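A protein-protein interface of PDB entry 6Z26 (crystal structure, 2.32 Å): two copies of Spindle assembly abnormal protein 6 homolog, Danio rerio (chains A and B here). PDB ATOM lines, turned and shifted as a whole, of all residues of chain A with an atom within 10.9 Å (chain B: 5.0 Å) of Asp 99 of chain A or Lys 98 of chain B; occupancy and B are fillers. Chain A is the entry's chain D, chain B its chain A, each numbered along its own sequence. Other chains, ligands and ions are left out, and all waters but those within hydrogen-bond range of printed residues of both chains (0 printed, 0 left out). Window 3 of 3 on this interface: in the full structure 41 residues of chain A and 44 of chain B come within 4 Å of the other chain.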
ATOM      1  N   LEU A  91     -11.766   5.218   4.812  1.00  0.00           N
ATOM      2  CA  LEU A  91     -10.328   5.250   4.518  1.00  0.00           C
ATOM      3  C   LEU A  91      -9.489   4.669   5.652  1.00  0.00           C
ATOM      4  O   LEU A  91      -8.535   3.946   5.382  1.00  0.00           O
ATOM      5  CB  LEU A  91      -9.871   6.684   4.150  1.00  0.00           C
ATOM      6  CG  LEU A  91     -10.526   7.319   2.916  1.00  0.00           C
ATOM      7  CD1 LEU A  91     -10.222   8.787   2.833  1.00  0.00           C
ATOM      8  CD2 LEU A  91     -10.092   6.627   1.634  1.00  0.00           C
ATOM      9  N   GLU A  92      -9.869   4.942   6.912  1.00  0.00           N
ATOM     10  CA  GLU A  92      -9.164   4.433   8.090  1.00  0.00           C
ATOM     11  C   GLU A  92      -9.220   2.913   8.185  1.00  0.00           C
ATOM     12  O   GLU A  92      -8.249   2.298   8.634  1.00  0.00           O
ATOM     13  CB  GLU A  92      -9.666   5.104   9.373  1.00  0.00           C
ATOM     14  CG  GLU A  92      -9.075   6.497   9.563  1.00  0.00           C
ATOM     15  CD  GLU A  92      -9.432   7.202  10.854  1.00  0.00           C
ATOM     16  OE1 GLU A  92     -10.567   7.007  11.348  1.00  0.00           O
ATOM     17  OE2 GLU A  92      -8.577   7.965  11.363  1.00  0.00           O
ATOM     18  N   GLN A  93     -10.344   2.311   7.721  1.00  0.00           N
ATOM     19  CA  GLN A  93     -10.540   0.869   7.667  1.00  0.00           C
ATOM     20  C   GLN A  93      -9.746   0.298   6.521  1.00  0.00           C
ATOM     21  O   GLN A  93      -9.128  -0.756   6.706  1.00  0.00           O
ATOM     22  CB  GLN A  93     -12.021   0.496   7.535  1.00  0.00           C
ATOM     23  CG  GLN A  93     -12.307  -1.018   7.692  1.00  0.00           C
ATOM     24  CD  GLN A  93     -11.954  -1.589   9.058  1.00  0.00           C
ATOM     25  OE1 GLN A  93     -12.366  -1.085  10.111  1.00  0.00           O
ATOM     26  NE2 GLN A  93     -11.174  -2.658   9.069  1.00  0.00           N
ATOM     27  N   GLU A  94      -9.734   0.985   5.336  1.00  0.00           N
ATOM     28  CA  GLU A  94      -8.951   0.535   4.162  1.00  0.00           C
ATOM     29  C   GLU A  94      -7.471   0.406   4.506  1.00  0.00           C
ATOM     30  O   GLU A  94      -6.827  -0.538   4.048  1.00  0.00           O
ATOM     31  CB  GLU A  94      -9.122   1.469   2.960  1.00  0.00           C
ATOM     32  CG  GLU A  94     -10.390   1.217   2.158  1.00  0.00           C
ATOM     33  CD  GLU A  94     -10.598   2.136   0.964  1.00  0.00           C
ATOM     34  OE1 GLU A  94     -11.738   2.626   0.795  1.00  0.00           O
ATOM     35  OE2 GLU A  94      -9.629   2.370   0.202  1.00  0.00           O
ATOM     36  N   ILE A  95      -6.949   1.330   5.342  1.00  0.00           N
ATOM     37  CA  ILE A  95      -5.564   1.349   5.822  1.00  0.00           C
ATOM     38  C   ILE A  95      -5.307   0.112   6.683  1.00  0.00           C
ATOM     39  O   ILE A  95      -4.395  -0.646   6.372  1.00  0.00           O
ATOM     40  CB  ILE A  95      -5.219   2.697   6.539  1.00  0.00           C
ATOM     41  CG1 ILE A  95      -5.163   3.830   5.511  1.00  0.00           C
ATOM     42  CG2 ILE A  95      -3.892   2.610   7.340  1.00  0.00           C
ATOM     43  CD1 ILE A  95      -5.151   5.187   6.081  1.00  0.00           C
ATOM     44  N   LYS A  96      -6.146  -0.114   7.719  1.00  0.00           N
ATOM     45  CA  LYS A  96      -6.066  -1.246   8.640  1.00  0.00           C
ATOM     46  C   LYS A  96      -6.030  -2.602   7.919  1.00  0.00           C
ATOM     47  O   LYS A  96      -5.199  -3.462   8.247  1.00  0.00           O
ATOM     48  CB  LYS A  96      -7.207  -1.202   9.670  1.00  0.00           C
ATOM     49  CG  LYS A  96      -6.877  -0.350  10.897  1.00  0.00           C
ATOM     50  CD  LYS A  96      -8.009  -0.393  11.882  1.00  0.00           C
ATOM     51  CE  LYS A  96      -7.772   0.497  13.056  1.00  0.00           C
ATOM     52  NZ  LYS A  96      -9.063   0.874  13.655  1.00  0.00           N
ATOM     53  N   ASP A  97      -6.913  -2.762   6.912  1.00  0.00           N
ATOM     54  CA  ASP A  97      -7.021  -3.964   6.081  1.00  0.00           C
ATOM     55  C   ASP A  97      -5.787  -4.174   5.205  1.00  0.00           C
ATOM     56  O   ASP A  97      -5.360  -5.317   5.029  1.00  0.00           O
ATOM     57  CB  ASP A  97      -8.296  -3.911   5.220  1.00  0.00           C
ATOM     58  CG  ASP A  97      -9.613  -3.898   5.999  1.00  0.00           C
ATOM     59  OD1 ASP A  97      -9.589  -4.177   7.225  1.00  0.00           O
ATOM     60  OD2 ASP A  97     -10.667  -3.616   5.380  1.00  0.00           O
ATOM     61  N   LYS A  98      -5.212  -3.082   4.665  1.00  0.00           N
ATOM     62  CA  LYS A  98      -4.012  -3.135   3.823  1.00  0.00           C
ATOM     63  C   LYS A  98      -2.766  -3.405   4.655  1.00  0.00           C
ATOM     64  O   LYS A  98      -1.923  -4.176   4.224  1.00  0.00           O
ATOM     65  CB  LYS A  98      -3.872  -1.881   2.942  1.00  0.00           C
ATOM     66  CG  LYS A  98      -4.817  -1.893   1.732  1.00  0.00           C
ATOM     67  CD  LYS A  98      -4.871  -0.546   1.025  1.00  0.00           C
ATOM     68  CE  LYS A  98      -6.195  -0.263   0.342  1.00  0.00           C
ATOM     69  NZ  LYS A  98      -6.297  -0.904  -0.991  1.00  0.00           N
ATOM     70  N   ASP A  99      -2.675  -2.823   5.867  1.00  0.00           N
ATOM     71  CA  ASP A  99      -1.564  -3.045   6.801  1.00  0.00           C
ATOM     72  C   ASP A  99      -1.501  -4.507   7.258  1.00  0.00           C
ATOM     73  O   ASP A  99      -0.407  -5.069   7.386  1.00  0.00           O
ATOM     74  CB  ASP A  99      -1.695  -2.115   8.017  1.00  0.00           C
ATOM     75  CG  ASP A  99      -1.337  -0.676   7.736  1.00  0.00           C
ATOM     76  OD1 ASP A  99      -0.650  -0.426   6.728  1.00  0.00           O
ATOM     77  OD2 ASP A  99      -1.739   0.202   8.534  1.00  0.00           O
ATOM     78  N   GLN A 100      -2.694  -5.107   7.497  1.00  0.00           N
ATOM     79  CA  GLN A 100      -2.882  -6.501   7.889  1.00  0.00           C
ATOM     80  C   GLN A 100      -2.506  -7.445   6.761  1.00  0.00           C
ATOM     81  O   GLN A 100      -1.956  -8.505   7.037  1.00  0.00           O
ATOM     82  CB  GLN A 100      -4.320  -6.755   8.336  1.00  0.00           C
ATOM     83  CG  GLN A 100      -4.440  -6.848   9.847  1.00  0.00           C
ATOM     84  CD  GLN A 100      -5.789  -7.367  10.247  1.00  0.00           C
ATOM     85  OE1 GLN A 100      -6.780  -6.619  10.259  1.00  0.00           O
ATOM     86  NE2 GLN A 100      -5.859  -8.661  10.588  1.00  0.00           N
ATOM     87  N   LEU A 101      -2.784  -7.057   5.493  1.00  0.00           N
ATOM     88  CA  LEU A 101      -2.407  -7.803   4.284  1.00  0.00           C
ATOM     89  C   LEU A 101      -0.886  -7.760   4.146  1.00  0.00           C
ATOM     90  O   LEU A 101      -0.284  -8.786   3.826  1.00  0.00           O
ATOM     91  CB  LEU A 101      -3.069  -7.196   3.036  1.00  0.00           C
ATOM     92  CG  LEU A 101      -3.067  -8.044   1.768  1.00  0.00           C
ATOM     93  CD1 LEU A 101      -4.248  -9.010   1.760  1.00  0.00           C
ATOM     94  CD2 LEU A 101      -3.112  -7.162   0.516  1.00  0.00           C
ATOM     95  N   VAL A 102      -0.264  -6.589   4.430  1.00  0.00           N
ATOM     96  CA  VAL A 102       1.192  -6.379   4.410  1.00  0.00           C
ATOM     97  C   VAL A 102       1.851  -7.208   5.528  1.00  0.00           C
ATOM     98  O   VAL A 102       2.928  -7.757   5.326  1.00  0.00           O
ATOM     99  CB  VAL A 102       1.569  -4.868   4.458  1.00  0.00           C
ATOM    100  CG1 VAL A 102       3.037  -4.649   4.842  1.00  0.00           C
ATOM    101  CG2 VAL A 102       1.262  -4.187   3.127  1.00  0.00           C
ATOM    102  N   LEU A 103       1.169  -7.344   6.670  1.00  0.00           N
ATOM    103  CA  LEU A 103       1.640  -8.128   7.811  1.00  0.00           C
ATOM    104  C   LEU A 103       1.613  -9.633   7.507  1.00  0.00           C
ATOM    105  O   LEU A 103       2.612 -10.317   7.741  1.00  0.00           O
ATOM    106  CB  LEU A 103       0.808  -7.798   9.062  1.00  0.00           C
ATOM    107  CG  LEU A 103       1.428  -8.105  10.431  1.00  0.00           C
ATOM    108  CD1 LEU A 103       2.667  -7.254  10.693  1.00  0.00           C
ATOM    109  CD2 LEU A 103       0.421  -7.874  11.546  1.00  0.00           C
ATOM    110  N   ARG A 104       0.491 -10.134   6.946  1.00  0.00           N
ATOM    111  CA  ARG A 104       0.333 -11.548   6.597  1.00  0.00           C
ATOM    112  C   ARG A 104       1.301 -12.002   5.487  1.00  0.00           C
ATOM    113  O   ARG A 104       1.741 -13.156   5.507  1.00  0.00           O
ATOM    114  CB  ARG A 104      -1.126 -11.886   6.269  1.00  0.00           C
ATOM    115  CG  ARG A 104      -1.976 -12.144   7.518  1.00  0.00           C
ATOM    116  CD  ARG A 104      -3.439 -12.417   7.209  1.00  0.00           C
ATOM    117  NE  ARG A 104      -3.625 -13.680   6.485  1.00  0.00           N
ATOM    118  CZ  ARG A 104      -4.793 -14.293   6.316  1.00  0.00           C
ATOM    119  NH1 ARG A 104      -5.905 -13.774   6.830  1.00  0.00           N
ATOM    120  NH2 ARG A 104      -4.860 -15.430   5.637  1.00  0.00           N
ATOM    121  N   THR A 105       1.664 -11.096   4.560  1.00  0.00           N
ATOM    122  CA  THR A 105       2.637 -11.384   3.500  1.00  0.00           C
ATOM    123  C   THR A 105       4.043 -11.502   4.113  1.00  0.00           C
ATOM    124  O   THR A 105       4.771 -12.437   3.773  1.00  0.00           O
ATOM    125  CB  THR A 105       2.575 -10.349   2.372  1.00  0.00           C
ATOM    126  OG1 THR A 105       2.504  -9.048   2.933  1.00  0.00           O
ATOM    127  CG2 THR A 105       1.406 -10.560   1.440  1.00  0.00           C
ATOM    128  N   LYS A 106       4.395 -10.584   5.048  1.00  0.00           N
ATOM    129  CA  LYS A 106       5.669 -10.593   5.775  1.00  0.00           C
ATOM    130  C   LYS A 106       5.804 -11.917   6.546  1.00  0.00           C
ATOM    131  O   LYS A 106       6.864 -12.547   6.488  1.00  0.00           O
ATOM    132  CB  LYS A 106       5.757  -9.411   6.768  1.00  0.00           C
ATOM    133  CG  LYS A 106       6.231  -8.096   6.180  1.00  0.00           C
ATOM    134  CD  LYS A 106       6.195  -6.971   7.212  1.00  0.00           C
ATOM    135  CE  LYS A 106       6.369  -5.609   6.575  1.00  0.00           C
ATOM    136  NZ  LYS A 106       6.063  -4.506   7.518  1.00  0.00           N
ATOM    137  N   GLU A 107       4.714 -12.334   7.243  1.00  0.00           N
ATOM    138  CA  GLU A 107       4.616 -13.557   8.050  1.00  0.00           C
ATOM    139  C   GLU A 107       4.828 -14.829   7.250  1.00  0.00           C
ATOM    140  O   GLU A 107       5.420 -15.771   7.781  1.00  0.00           O
ATOM    141  CB  GLU A 107       3.259 -13.643   8.761  1.00  0.00           C
ATOM    142  CG  GLU A 107       3.091 -12.676   9.916  1.00  0.00           C
ATOM    143  CD  GLU A 107       1.752 -12.749  10.619  1.00  0.00           C
ATOM    144  OE1 GLU A 107       0.732 -13.082   9.968  1.00  0.00           O
ATOM    145  OE2 GLU A 107       1.742 -12.526  11.850  1.00  0.00           O
ATOM    146  N   GLU B  94      -1.675   7.731   2.140  1.00  0.00           N
ATOM    147  CA  GLU B  94      -1.189   6.541   2.860  1.00  0.00           C
ATOM    148  C   GLU B  94      -1.568   5.257   2.117  1.00  0.00           C
ATOM    149  O   GLU B  94      -0.766   4.312   2.055  1.00  0.00           O
ATOM    150  CB  GLU B  94      -1.742   6.496   4.292  1.00  0.00           C
ATOM    151  CG  GLU B  94      -0.966   7.360   5.267  1.00  0.00           C
ATOM    152  CD  GLU B  94      -1.463   7.412   6.700  1.00  0.00           C
ATOM    153  OE1 GLU B  94      -2.141   6.460   7.158  1.00  0.00           O
ATOM    154  OE2 GLU B  94      -1.161   8.425   7.371  1.00  0.00           O
ATOM    155  N   ILE B  95      -2.785   5.246   1.526  1.00  0.00           N
ATOM    156  CA  ILE B  95      -3.328   4.133   0.743  1.00  0.00           C
ATOM    157  C   ILE B  95      -2.490   3.938  -0.513  1.00  0.00           C
ATOM    158  O   ILE B  95      -1.973   2.841  -0.709  1.00  0.00           O
ATOM    159  CB  ILE B  95      -4.859   4.301   0.480  1.00  0.00           C
ATOM    160  CG1 ILE B  95      -5.658   4.141   1.807  1.00  0.00           C
ATOM    161  CG2 ILE B  95      -5.370   3.341  -0.611  1.00  0.00           C
ATOM    162  CD1 ILE B  95      -7.028   4.563   1.785  1.00  0.00           C
ATOM    163  N   LYS B  96      -2.304   5.015  -1.323  1.00  0.00           N
ATOM    164  CA  LYS B  96      -1.502   5.021  -2.556  1.00  0.00           C
ATOM    165  C   LYS B  96      -0.091   4.475  -2.336  1.00  0.00           C
ATOM    166  O   LYS B  96       0.363   3.666  -3.139  1.00  0.00           O
ATOM    167  CB  LYS B  96      -1.437   6.422  -3.177  1.00  0.00           C
ATOM    168  CG  LYS B  96      -2.574   6.727  -4.140  1.00  0.00           C
ATOM    169  CD  LYS B  96      -2.417   8.129  -4.744  1.00  0.00           C
ATOM    170  CE  LYS B  96      -3.619   8.619  -5.528  1.00  0.00           C
ATOM    171  NZ  LYS B  96      -4.632   9.300  -4.659  1.00  0.00           N
ATOM    172  N   ASP B  97       0.579   4.896  -1.238  1.00  0.00           N
ATOM    173  CA  ASP B  97       1.933   4.469  -0.863  1.00  0.00           C
ATOM    174  C   ASP B  97       2.000   2.977  -0.481  1.00  0.00           C
ATOM    175  O   ASP B  97       2.971   2.289  -0.827  1.00  0.00           O
ATOM    176  CB  ASP B  97       2.485   5.349   0.269  1.00  0.00           C
ATOM    177  CG  ASP B  97       2.655   6.823  -0.067  1.00  0.00           C
ATOM    178  OD1 ASP B  97       2.553   7.182  -1.263  1.00  0.00           O
ATOM    179  OD2 ASP B  97       2.903   7.617   0.866  1.00  0.00           O
ATOM    180  N   LYS B  98       0.964   2.488   0.221  1.00  0.00           N
ATOM    181  CA  LYS B  98       0.876   1.087   0.634  1.00  0.00           C
ATOM    182  C   LYS B  98       0.523   0.180  -0.551  1.00  0.00           C
ATOM    183  O   LYS B  98       1.086  -0.908  -0.668  1.00  0.00           O
ATOM    184  CB  LYS B  98      -0.093   0.916   1.819  1.00  0.00           C
ATOM    185  CG  LYS B  98       0.487   1.405   3.155  1.00  0.00           C
ATOM    186  CD  LYS B  98      -0.576   1.524   4.251  1.00  0.00           C
ATOM    187  CE  LYS B  98      -0.268   2.577   5.301  1.00  0.00           C
ATOM    188  NZ  LYS B  98       0.709   2.108   6.319  1.00  0.00           N
ATOM    189  N   ASP B  99      -0.369   0.644  -1.450  1.00  0.00           N
ATOM    190  CA  ASP B  99      -0.753  -0.087  -2.663  1.00  0.00           C
ATOM    191  C   ASP B  99       0.437  -0.234  -3.614  1.00  0.00           C
ATOM    192  O   ASP B  99       0.582  -1.284  -4.247  1.00  0.00           O
ATOM    193  CB  ASP B  99      -1.890   0.628  -3.392  1.00  0.00           C
ATOM    194  CG  ASP B  99      -3.242   0.500  -2.736  1.00  0.00           C
ATOM    195  OD1 ASP B  99      -3.411  -0.411  -1.897  1.00  0.00           O
ATOM    196  OD2 ASP B  99      -4.140   1.299  -3.074  1.00  0.00           O
ATOM    197  N   GLN B 100       1.284   0.825  -3.710  1.00  0.00           N
ATOM    198  CA  GLN B 100       2.507   0.878  -4.526  1.00  0.00           C
ATOM    199  C   GLN B 100       3.554  -0.094  -3.976  1.00  0.00           C
ATOM    200  O   GLN B 100       4.267  -0.713  -4.767  1.00  0.00           O
ATOM    201  CB  GLN B 100       3.107   2.301  -4.595  1.00  0.00           C
ATOM    202  CG  GLN B 100       2.495   3.342  -5.567  1.00  0.00           C
ATOM    203  CD  GLN B 100       2.051   2.875  -6.929  1.00  0.00           C
ATOM    204  OE1 GLN B 100       2.850   2.385  -7.726  1.00  0.00           O
ATOM    205  NE2 GLN B 100       0.765   3.015  -7.207  1.00  0.00           N
ATOM    206  N   LEU B 101       3.638  -0.230  -2.633  1.00  0.00           N
ATOM    207  CA  LEU B 101       4.531  -1.171  -1.954  1.00  0.00           C
ATOM    208  C   LEU B 101       4.063  -2.609  -2.256  1.00  0.00           C
ATOM    209  O   LEU B 101       4.892  -3.470  -2.550  1.00  0.00           O
ATOM    210  CB  LEU B 101       4.536  -0.918  -0.435  1.00  0.00           C
ATOM    211  CG  LEU B 101       5.630  -1.641   0.375  1.00  0.00           C
ATOM    212  CD1 LEU B 101       6.948  -0.865   0.344  1.00  0.00           C
ATOM    213  CD2 LEU B 101       5.194  -1.838   1.817  1.00  0.00           C
ATOM    214  N   VAL B 102       2.725  -2.835  -2.230  1.00  0.00           N
ATOM    215  CA  VAL B 102       2.074  -4.113  -2.546  1.00  0.00           C
ATOM    216  C   VAL B 102       2.295  -4.448  -4.028  1.00  0.00           C
ATOM    217  O   VAL B 102       2.490  -5.609  -4.367  1.00  0.00           O
ATOM    218  CB  VAL B 102       0.575  -4.121  -2.119  1.00  0.00           C
ATOM    219  CG1 VAL B 102      -0.218  -5.239  -2.791  1.00  0.00           C
ATOM    220  CG2 VAL B 102       0.438  -4.219  -0.605  1.00  0.00           C
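The side-chain amino group of Lys 98 of chain B lies within salt-bridge range of the side-chain carboxylate of Asp 99 of chain A (2.9 Å).
OD1 of Asp 99 of chain B is in salt-bridge range of NZ of Lys 98 of chain A.
Glu 94 of chain A touches Ile 95 of chain B, and with the chains exchanged Ile 95 of chain A touches Glu 94 of chain B.
Lys 98 of chain A touches Ile 95 of chain B, but with the chains exchanged Ile 95 of chain A does not touch Lys 98 of chain B (4.2 Å).
Lys 98 of chain A touches Asp 99 of chain B, and with the chains exchanged Asp 99 of chain A touches Lys 98 of chain B.
Val 102 of chain A touches its own counterpart, Val 102 of chain B.
Positions printed for both chains: 94, 95, 96, 97, 98, 99, 100, 101 and 102.
Of the printed residues of chain B, Asp 99 of chain A touches Lys 98.
Lys 98 of chain B touches one residue of chain A.
No residue of chain A comes within 4 Å of Asp 97 of chain B.
Asp 99 of chain B touches one residue of chain A.
No residue of chain A comes within 4 Å of Leu 101 of chain B.
Of the printed residues of chain A, Val 102 of chain B touches Val 102 (3.8 Å).
Printed residues of chain B within 4 Å of Leu 91 of chain A: Ile 95 (3.7 Å).
Of the printed residues of chain B, Glu 94 of chain A touches Ile 95 (3.8 Å).
Of the printed residues of chain B, Lys 98 of chain A touches Ile 95 and Asp 99.
Asp 97 of chain A touches none of the printed residues of chain B.
The nearest residue of chain A that does not touch Lys 98 of chain B is Ile 95 of chain A (4.2 Å).
O of Val 102 of chain A sits at hydrogen-bond distance from OG1 of Thr 105 of chain A (2.8 Å).
Of the 9 printed residues of chain B, 5 touch a printed residue of chain A.
Printed residues of chain B that touch a printed residue of chain A: Glu 94, Ile 95, Lys 98, Asp 99 and Val 102.
Of the 17 printed residues of chain A, 6 touch a printed residue of chain B.
Hydrophobic or aromatic side chains of chain A within 4 Å of the printed part of chain B: Leu 91, Ile 95 and Val 102.
Along chain A the printed residues that touch a printed residue of chain B span positions 91 to 102.
Among the printed residues, Asp or Glu carboxylates within 4 Å of a Lys or Arg side-chain nitrogen of the other chain: Lys 98 of chain A with Asp 99 of chain B (3.1 Å) and Asp 99 of chain A with Lys 98 of chain B (2.9 Å).
Leu 91 of chain A touches Ile 95 of chain B (CD2 to CD1, 3.7 Å).
CD1 of Ile 95 of chain B touches OE2 of Glu 94 of chain A (3.8 Å).
Ile 95 of chain A touches Glu 94 of chain B (CD1 to OE1, 3.4 Å).
CG1 of Ile 95 of chain B touches CG1 of Ile 95 of chain A (3.7 Å).
Ile 95 of chain B touches Lys 98 of chain A.
Val 102 of chain B touches Val 102 of chain A (CG2 to CG2, 3.8 Å).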
